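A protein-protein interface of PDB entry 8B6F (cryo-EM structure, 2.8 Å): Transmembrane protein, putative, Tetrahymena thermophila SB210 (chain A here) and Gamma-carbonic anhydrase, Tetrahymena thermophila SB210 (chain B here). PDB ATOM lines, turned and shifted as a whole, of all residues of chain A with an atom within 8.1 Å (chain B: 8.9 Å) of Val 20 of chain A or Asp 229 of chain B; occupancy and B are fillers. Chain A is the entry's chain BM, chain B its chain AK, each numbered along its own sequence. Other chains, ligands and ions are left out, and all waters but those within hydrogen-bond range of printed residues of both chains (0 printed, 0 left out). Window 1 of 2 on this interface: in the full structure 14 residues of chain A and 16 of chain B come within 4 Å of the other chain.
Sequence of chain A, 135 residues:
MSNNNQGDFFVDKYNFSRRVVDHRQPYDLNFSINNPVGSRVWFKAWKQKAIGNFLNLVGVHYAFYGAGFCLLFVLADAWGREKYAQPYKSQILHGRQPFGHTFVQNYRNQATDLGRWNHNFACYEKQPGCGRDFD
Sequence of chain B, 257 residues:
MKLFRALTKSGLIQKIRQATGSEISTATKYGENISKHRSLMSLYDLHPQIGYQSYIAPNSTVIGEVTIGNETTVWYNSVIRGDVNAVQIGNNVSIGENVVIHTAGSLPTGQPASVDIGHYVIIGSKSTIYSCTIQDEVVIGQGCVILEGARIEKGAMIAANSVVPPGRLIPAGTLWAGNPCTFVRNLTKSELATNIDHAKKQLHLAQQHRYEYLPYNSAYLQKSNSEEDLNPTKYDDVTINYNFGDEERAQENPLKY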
ATOM      1  N   SER A  17      -9.301  19.811 -13.590  1.00  0.00           N
ATOM      2  CA  SER A  17      -9.415  18.381 -13.337  1.00  0.00           C
ATOM      3  C   SER A  17     -10.452  18.074 -12.262  1.00  0.00           C
ATOM      4  O   SER A  17     -10.450  16.976 -11.700  1.00  0.00           O
ATOM      5  CB  SER A  17      -8.057  17.800 -12.947  1.00  0.00           C
ATOM      6  OG  SER A  17      -7.580  18.382 -11.748  1.00  0.00           O
ATOM      7  N   ARG A  18     -11.333  19.026 -11.963  1.00  0.00           N
ATOM      8  CA  ARG A  18     -12.373  18.797 -10.969  1.00  0.00           C
ATOM      9  C   ARG A  18     -13.209  17.587 -11.358  1.00  0.00           C
ATOM     10  O   ARG A  18     -13.576  17.414 -12.522  1.00  0.00           O
ATOM     11  CB  ARG A  18     -13.265  20.033 -10.847  1.00  0.00           C
ATOM     12  CG  ARG A  18     -14.265  19.976  -9.702  1.00  0.00           C
ATOM     13  CD  ARG A  18     -13.589  20.229  -8.369  1.00  0.00           C
ATOM     14  NE  ARG A  18     -14.525  20.141  -7.255  1.00  0.00           N
ATOM     15  CZ  ARG A  18     -14.769  19.040  -6.558  1.00  0.00           C
ATOM     16  NH1 ARG A  18     -14.164  17.896  -6.834  1.00  0.00           N
ATOM     17  NH2 ARG A  18     -15.639  19.087  -5.554  1.00  0.00           N
ATOM     18  N   ARG A  19     -13.508  16.741 -10.376  1.00  0.00           N
ATOM     19  CA  ARG A  19     -14.257  15.522 -10.650  1.00  0.00           C
ATOM     20  C   ARG A  19     -14.836  14.973  -9.357  1.00  0.00           C
ATOM     21  O   ARG A  19     -14.103  14.770  -8.386  1.00  0.00           O
ATOM     22  CB  ARG A  19     -13.359  14.477 -11.321  1.00  0.00           C
ATOM     23  CG  ARG A  19     -14.015  13.119 -11.491  1.00  0.00           C
ATOM     24  CD  ARG A  19     -13.201  12.215 -12.401  1.00  0.00           C
ATOM     25  NE  ARG A  19     -13.787  10.884 -12.500  1.00  0.00           N
ATOM     26  CZ  ARG A  19     -14.857  10.586 -13.225  1.00  0.00           C
ATOM     27  NH1 ARG A  19     -15.499  11.507 -13.924  1.00  0.00           N
ATOM     28  NH2 ARG A  19     -15.297   9.331 -13.246  1.00  0.00           N
ATOM     29  N   VAL A  20     -16.145  14.738  -9.353  1.00  0.00           N
ATOM     30  CA  VAL A  20     -16.828  14.049  -8.265  1.00  0.00           C
ATOM     31  C   VAL A  20     -17.584  12.879  -8.880  1.00  0.00           C
ATOM     32  O   VAL A  20     -18.444  13.080  -9.744  1.00  0.00           O
ATOM     33  CB  VAL A  20     -17.787  14.974  -7.498  1.00  0.00           C
ATOM     34  CG1 VAL A  20     -18.424  14.234  -6.331  1.00  0.00           C
ATOM     35  CG2 VAL A  20     -17.059  16.211  -7.012  1.00  0.00           C
ATOM     36  N   VAL A  21     -17.268  11.663  -8.435  1.00  0.00           N
ATOM     37  CA  VAL A  21     -17.853  10.473  -9.037  1.00  0.00           C
ATOM     38  C   VAL A  21     -19.317  10.358  -8.640  1.00  0.00           C
ATOM     39  O   VAL A  21     -19.692  10.603  -7.485  1.00  0.00           O
ATOM     40  CB  VAL A  21     -17.062   9.220  -8.625  1.00  0.00           C
ATOM     41  CG1 VAL A  21     -17.755   7.953  -9.109  1.00  0.00           C
ATOM     42  CG2 VAL A  21     -15.652   9.290  -9.175  1.00  0.00           C
ATOM     43  N   ASP A  22     -20.153   9.976  -9.602  1.00  0.00           N
ATOM     44  CA  ASP A  22     -21.585   9.830  -9.370  1.00  0.00           C
ATOM     45  C   ASP A  22     -21.842   8.558  -8.572  1.00  0.00           C
ATOM     46  O   ASP A  22     -21.686   7.447  -9.090  1.00  0.00           O
ATOM     47  CB  ASP A  22     -22.325   9.799 -10.704  1.00  0.00           C
ATOM     48  CG  ASP A  22     -23.826   9.839 -10.540  1.00  0.00           C
ATOM     49  OD1 ASP A  22     -24.296  10.036  -9.401  1.00  0.00           O
ATOM     50  OD2 ASP A  22     -24.538   9.670 -11.552  1.00  0.00           O
ATOM     51  N   HIS A  23     -22.236   8.716  -7.309  1.00  0.00           N
ATOM     52  CA  HIS A  23     -22.499   7.575  -6.443  1.00  0.00           C
ATOM     53  C   HIS A  23     -23.812   6.877  -6.767  1.00  0.00           C
ATOM     54  O   HIS A  23     -24.062   5.793  -6.231  1.00  0.00           O
ATOM     55  CB  HIS A  23     -22.514   8.021  -4.981  1.00  0.00           C
ATOM     56  CG  HIS A  23     -23.644   8.944  -4.646  1.00  0.00           C
ATOM     57  ND1 HIS A  23     -23.682  10.259  -5.058  1.00  0.00           N
ATOM     58  CD2 HIS A  23     -24.778   8.741  -3.935  1.00  0.00           C
ATOM     59  CE1 HIS A  23     -24.790  10.824  -4.618  1.00  0.00           C
ATOM     60  NE2 HIS A  23     -25.474   9.926  -3.932  1.00  0.00           N
ATOM     61  N   TYR B 220     -18.227  25.286  -7.550  1.00  0.00           N
ATOM     62  CA  TYR B 220     -17.723  23.917  -7.532  1.00  0.00           C
ATOM     63  C   TYR B 220     -16.429  23.785  -8.324  1.00  0.00           C
ATOM     64  O   TYR B 220     -15.617  22.900  -8.040  1.00  0.00           O
ATOM     65  CB  TYR B 220     -18.778  22.960  -8.086  1.00  0.00           C
ATOM     66  CG  TYR B 220     -18.955  23.043  -9.584  1.00  0.00           C
ATOM     67  CD1 TYR B 220     -19.762  24.016 -10.157  1.00  0.00           C
ATOM     68  CD2 TYR B 220     -18.318  22.142 -10.425  1.00  0.00           C
ATOM     69  CE1 TYR B 220     -19.925  24.091 -11.527  1.00  0.00           C
ATOM     70  CE2 TYR B 220     -18.475  22.208 -11.794  1.00  0.00           C
ATOM     71  CZ  TYR B 220     -19.279  23.183 -12.338  1.00  0.00           C
ATOM     72  OH  TYR B 220     -19.436  23.251 -13.703  1.00  0.00           O
ATOM     73  N   LEU B 221     -16.220  24.648  -9.317  1.00  0.00           N
ATOM     74  CA  LEU B 221     -15.012  24.591 -10.127  1.00  0.00           C
ATOM     75  C   LEU B 221     -13.767  25.021  -9.366  1.00  0.00           C
ATOM     76  O   LEU B 221     -12.658  24.828  -9.872  1.00  0.00           O
ATOM     77  CB  LEU B 221     -15.179  25.469 -11.367  1.00  0.00           C
ATOM     78  CG  LEU B 221     -16.232  25.012 -12.376  1.00  0.00           C
ATOM     79  CD1 LEU B 221     -16.459  26.075 -13.433  1.00  0.00           C
ATOM     80  CD2 LEU B 221     -15.810  23.711 -13.022  1.00  0.00           C
ATOM     81  N   LYS B 223     -12.993  24.022  -6.151  1.00  0.00           N
ATOM     82  CA  LYS B 223     -12.644  23.071  -5.108  1.00  0.00           C
ATOM     83  C   LYS B 223     -11.632  22.054  -5.622  1.00  0.00           C
ATOM     84  O   LYS B 223     -11.463  21.859  -6.827  1.00  0.00           O
ATOM     85  CB  LYS B 223     -13.890  22.350  -4.596  1.00  0.00           C
ATOM     86  CG  LYS B 223     -14.856  23.244  -3.841  1.00  0.00           C
ATOM     87  CD  LYS B 223     -16.053  22.468  -3.316  1.00  0.00           C
ATOM     88  CE  LYS B 223     -15.652  21.466  -2.245  1.00  0.00           C
ATOM     89  NZ  LYS B 223     -16.840  20.808  -1.633  1.00  0.00           N
ATOM     90  N   SER B 224     -10.958  21.399  -4.682  1.00  0.00           N
ATOM     91  CA  SER B 224      -9.963  20.382  -4.988  1.00  0.00           C
ATOM     92  C   SER B 224     -10.554  18.994  -4.787  1.00  0.00           C
ATOM     93  O   SER B 224     -11.263  18.745  -3.810  1.00  0.00           O
ATOM     94  CB  SER B 224      -8.724  20.548  -4.106  1.00  0.00           C
ATOM     95  OG  SER B 224      -8.108  21.805  -4.321  1.00  0.00           O
ATOM     96  N   ASN B 225     -10.258  18.093  -5.722  1.00  0.00           N
ATOM     97  CA  ASN B 225     -10.763  16.730  -5.626  1.00  0.00           C
ATOM     98  C   ASN B 225     -10.253  16.063  -4.355  1.00  0.00           C
ATOM     99  O   ASN B 225      -9.092  16.219  -3.973  1.00  0.00           O
ATOM    100  CB  ASN B 225     -10.333  15.922  -6.848  1.00  0.00           C
ATOM    101  CG  ASN B 225     -10.901  16.470  -8.136  1.00  0.00           C
ATOM    102  OD1 ASN B 225     -12.036  16.942  -8.174  1.00  0.00           O
ATOM    103  ND2 ASN B 225     -10.112  16.417  -9.201  1.00  0.00           N
ATOM    104  N   SER B 226     -11.135  15.316  -3.701  1.00  0.00           N
ATOM    105  CA  SER B 226     -10.816  14.591  -2.481  1.00  0.00           C
ATOM    106  C   SER B 226     -10.986  13.097  -2.718  1.00  0.00           C
ATOM    107  O   SER B 226     -11.492  12.658  -3.753  1.00  0.00           O
ATOM    108  CB  SER B 226     -11.701  15.054  -1.316  1.00  0.00           C
ATOM    109  OG  SER B 226     -13.074  14.860  -1.606  1.00  0.00           O
ATOM    110  N   GLU B 227     -10.547  12.308  -1.736  1.00  0.00           N
ATOM    111  CA  GLU B 227     -10.670  10.858  -1.847  1.00  0.00           C
ATOM    112  C   GLU B 227     -12.134  10.441  -1.936  1.00  0.00           C
ATOM    113  O   GLU B 227     -12.488   9.556  -2.723  1.00  0.00           O
ATOM    114  CB  GLU B 227      -9.977  10.174  -0.665  1.00  0.00           C
ATOM    115  CG  GLU B 227     -10.714  10.253   0.673  1.00  0.00           C
ATOM    116  CD  GLU B 227     -10.888  11.674   1.173  1.00  0.00           C
ATOM    117  OE1 GLU B 227     -10.260  12.589   0.601  1.00  0.00           O
ATOM    118  OE2 GLU B 227     -11.651  11.877   2.139  1.00  0.00           O
ATOM    119  N   GLU B 228     -13.001  11.073  -1.143  1.00  0.00           N
ATOM    120  CA  GLU B 228     -14.426  10.763  -1.216  1.00  0.00           C
ATOM    121  C   GLU B 228     -14.994  11.113  -2.585  1.00  0.00           C
ATOM    122  O   GLU B 228     -15.793  10.355  -3.146  1.00  0.00           O
ATOM    123  CB  GLU B 228     -15.179  11.511  -0.116  1.00  0.00           C
ATOM    124  CG  GLU B 228     -16.674  11.220  -0.073  1.00  0.00           C
ATOM    125  CD  GLU B 228     -16.981   9.766   0.229  1.00  0.00           C
ATOM    126  OE1 GLU B 228     -16.081   9.058   0.727  1.00  0.00           O
ATOM    127  OE2 GLU B 228     -18.121   9.329  -0.033  1.00  0.00           O
ATOM    128  N   ASP B 229     -14.594  12.258  -3.140  1.00  0.00           N
ATOM    129  CA  ASP B 229     -15.084  12.645  -4.459  1.00  0.00           C
ATOM    130  C   ASP B 229     -14.641  11.652  -5.525  1.00  0.00           C
ATOM    131  O   ASP B 229     -15.420  11.301  -6.418  1.00  0.00           O
ATOM    132  CB  ASP B 229     -14.592  14.048  -4.808  1.00  0.00           C
ATOM    133  CG  ASP B 229     -15.087  15.099  -3.837  1.00  0.00           C
ATOM    134  OD1 ASP B 229     -15.762  14.728  -2.854  1.00  0.00           O
ATOM    135  OD2 ASP B 229     -14.805  16.295  -4.056  1.00  0.00           O
ATOM    136  N   LEU B 230     -13.391  11.194  -5.452  1.00  0.00           N
ATOM    137  CA  LEU B 230     -12.866  10.302  -6.479  1.00  0.00           C
ATOM    138  C   LEU B 230     -13.383   8.877  -6.332  1.00  0.00           C
ATOM    139  O   LEU B 230     -13.482   8.158  -7.331  1.00  0.00           O
ATOM    140  CB  LEU B 230     -11.337  10.313  -6.441  1.00  0.00           C
ATOM    141  CG  LEU B 230     -10.681  11.664  -6.747  1.00  0.00           C
ATOM    142  CD1 LEU B 230      -9.176  11.585  -6.555  1.00  0.00           C
ATOM    143  CD2 LEU B 230     -11.012  12.130  -8.156  1.00  0.00           C
ATOM    144  N   ASN B 231     -13.700   8.441  -5.113  1.00  0.00           N
ATOM    145  CA  ASN B 231     -14.184   7.083  -4.872  1.00  0.00           C
ATOM    146  C   ASN B 231     -15.250   7.115  -3.781  1.00  0.00           C
ATOM    147  O   ASN B 231     -14.922   7.240  -2.589  1.00  0.00           O
ATOM    148  CB  ASN B 231     -13.041   6.146  -4.492  1.00  0.00           C
ATOM    149  CG  ASN B 231     -12.200   6.681  -3.351  1.00  0.00           C
ATOM    150  OD1 ASN B 231     -12.494   6.436  -2.181  1.00  0.00           O
ATOM    151  ND2 ASN B 231     -11.143   7.409  -3.686  1.00  0.00           N
ATOM    152  N   PRO B 232     -16.529   7.009  -4.141  1.00  0.00           N
ATOM    153  CA  PRO B 232     -17.578   6.990  -3.115  1.00  0.00           C
ATOM    154  C   PRO B 232     -17.451   5.781  -2.200  1.00  0.00           C
ATOM    155  O   PRO B 232     -17.032   4.699  -2.615  1.00  0.00           O
ATOM    156  CB  PRO B 232     -18.877   6.937  -3.929  1.00  0.00           C
ATOM    157  CG  PRO B 232     -18.507   7.405  -5.289  1.00  0.00           C
ATOM    158  CD  PRO B 232     -17.095   6.971  -5.499  1.00  0.00           C
ATOM    159  N   THR B 233     -17.821   5.980  -0.934  1.00  0.00           N
ATOM    160  CA  THR B 233     -17.810   4.874   0.017  1.00  0.00           C
ATOM    161  C   THR B 233     -18.950   3.900  -0.256  1.00  0.00           C
ATOM    162  O   THR B 233     -18.748   2.679  -0.243  1.00  0.00           O
ATOM    163  CB  THR B 233     -17.903   5.411   1.446  1.00  0.00           C
ATOM    164  OG1 THR B 233     -16.824   6.323   1.690  1.00  0.00           O
ATOM    165  CG2 THR B 233     -17.837   4.273   2.458  1.00  0.00           C
ATOM    166  N   TYR B 235     -22.753   3.284  -2.704  1.00  0.00           N
ATOM    167  CA  TYR B 235     -23.467   3.639  -3.919  1.00  0.00           C
ATOM    168  C   TYR B 235     -24.968   3.491  -3.714  1.00  0.00           C
ATOM    169  O   TYR B 235     -25.429   2.638  -2.951  1.00  0.00           O
ATOM    170  CB  TYR B 235     -23.018   2.768  -5.096  1.00  0.00           C
ATOM    171  CG  TYR B 235     -21.599   3.035  -5.538  1.00  0.00           C
ATOM    172  CD1 TYR B 235     -20.524   2.459  -4.877  1.00  0.00           C
ATOM    173  CD2 TYR B 235     -21.337   3.860  -6.622  1.00  0.00           C
ATOM    174  CE1 TYR B 235     -19.225   2.702  -5.280  1.00  0.00           C
ATOM    175  CE2 TYR B 235     -20.044   4.110  -7.033  1.00  0.00           C
ATOM    176  CZ  TYR B 235     -18.993   3.526  -6.360  1.00  0.00           C
ATOM    177  OH  TYR B 235     -17.703   3.774  -6.767  1.00  0.00           O
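Of chain B, only Asp 229 comes within 4 Å of Val 20 of chain A.
Of the printed residues of chain A, Asp 229 of chain B touches Arg 18 (3.3 Å), Arg 19 (3.7 Å), Val 20 (3.6 Å) and Val 21 (2.8 Å).
Of the printed residues of chain B, Arg 18 of chain A touches Tyr 220 (3.1 Å), Lys 223 (3.1 Å), Asn 225 (2.7 Å) and Asp 229 (3.3 Å).
Of the printed residues of chain A, Tyr 220 of chain B touches Arg 18 (3.1 Å).
Of the printed residues of chain A, Pro 232 of chain B touches Val 21 and His 23.
Of the printed residues of chain A, Leu 230 of chain B touches Val 21.
The nearest residue of chain A that does not touch Asp 229 of chain B is Asp 22 of chain A (5.9 Å).
The backbone carbonyl oxygen (O) of Tyr 220 of chain B lies within hydrogen-bond range of the guanidinium group (NE) of Arg 18 of chain A.
ND2 of Asn 225 of chain B sits at hydrogen-bond distance from O of Ser 17 of chain A (2.6 Å).
The side-chain amide oxygen (OD1) of Asn 225 of chain B is in hydrogen-bond range of the guanidinium group (NH1) of Arg 18 of chain A, 2.7 Å away.
OD1 of Asn 225 of chain B is in hydrogen-bond range of N of Arg 19 of chain A, 2.7 Å away.
OD2 of Asp 229 of chain B lies within salt-bridge range of NH1 of Arg 18 of chain A (3.3 Å).
N of Val 21 of chain A is in hydrogen-bond range of O of Asp 229 of chain B.
Of the 7 printed residues of chain A, 6 touch a printed residue of chain B.
Of the 14 printed residues of chain B, 7 touch a printed residue of chain A.
Hydrophobic or aromatic side chains of chain B within 4 Å of the printed part of chain A: Pro 232 and Tyr 235.
Among the printed residues, Asp or Glu carboxylates within 4 Å of a Lys or Arg side-chain nitrogen of the other chain: Arg 18 of chain A with Asp 229 of chain B (3.3 Å).
Among the printed residues, pairs that only touch across the chains: Arg 18 of chain A with Lys 223 of chain B (3.1 Å), Arg 19 of chain A with Asp 229 of chain B (3.7 Å), Val 20 of chain A with Asp 229 of chain B (3.6 Å), Val 21 of chain A with Leu 230 of chain B (3.1 Å), Val 21 of chain A with Pro 232 of chain B (3.8 Å), His 23 of chain A with Pro 232 of chain B (3.9 Å) and His 23 of chain A with Tyr 235 of chain B (3.2 Å).
OD1 of Asp 229 of chain B is in hydrogen-bond range of OG of Ser 226 of chain B (3.0 Å).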
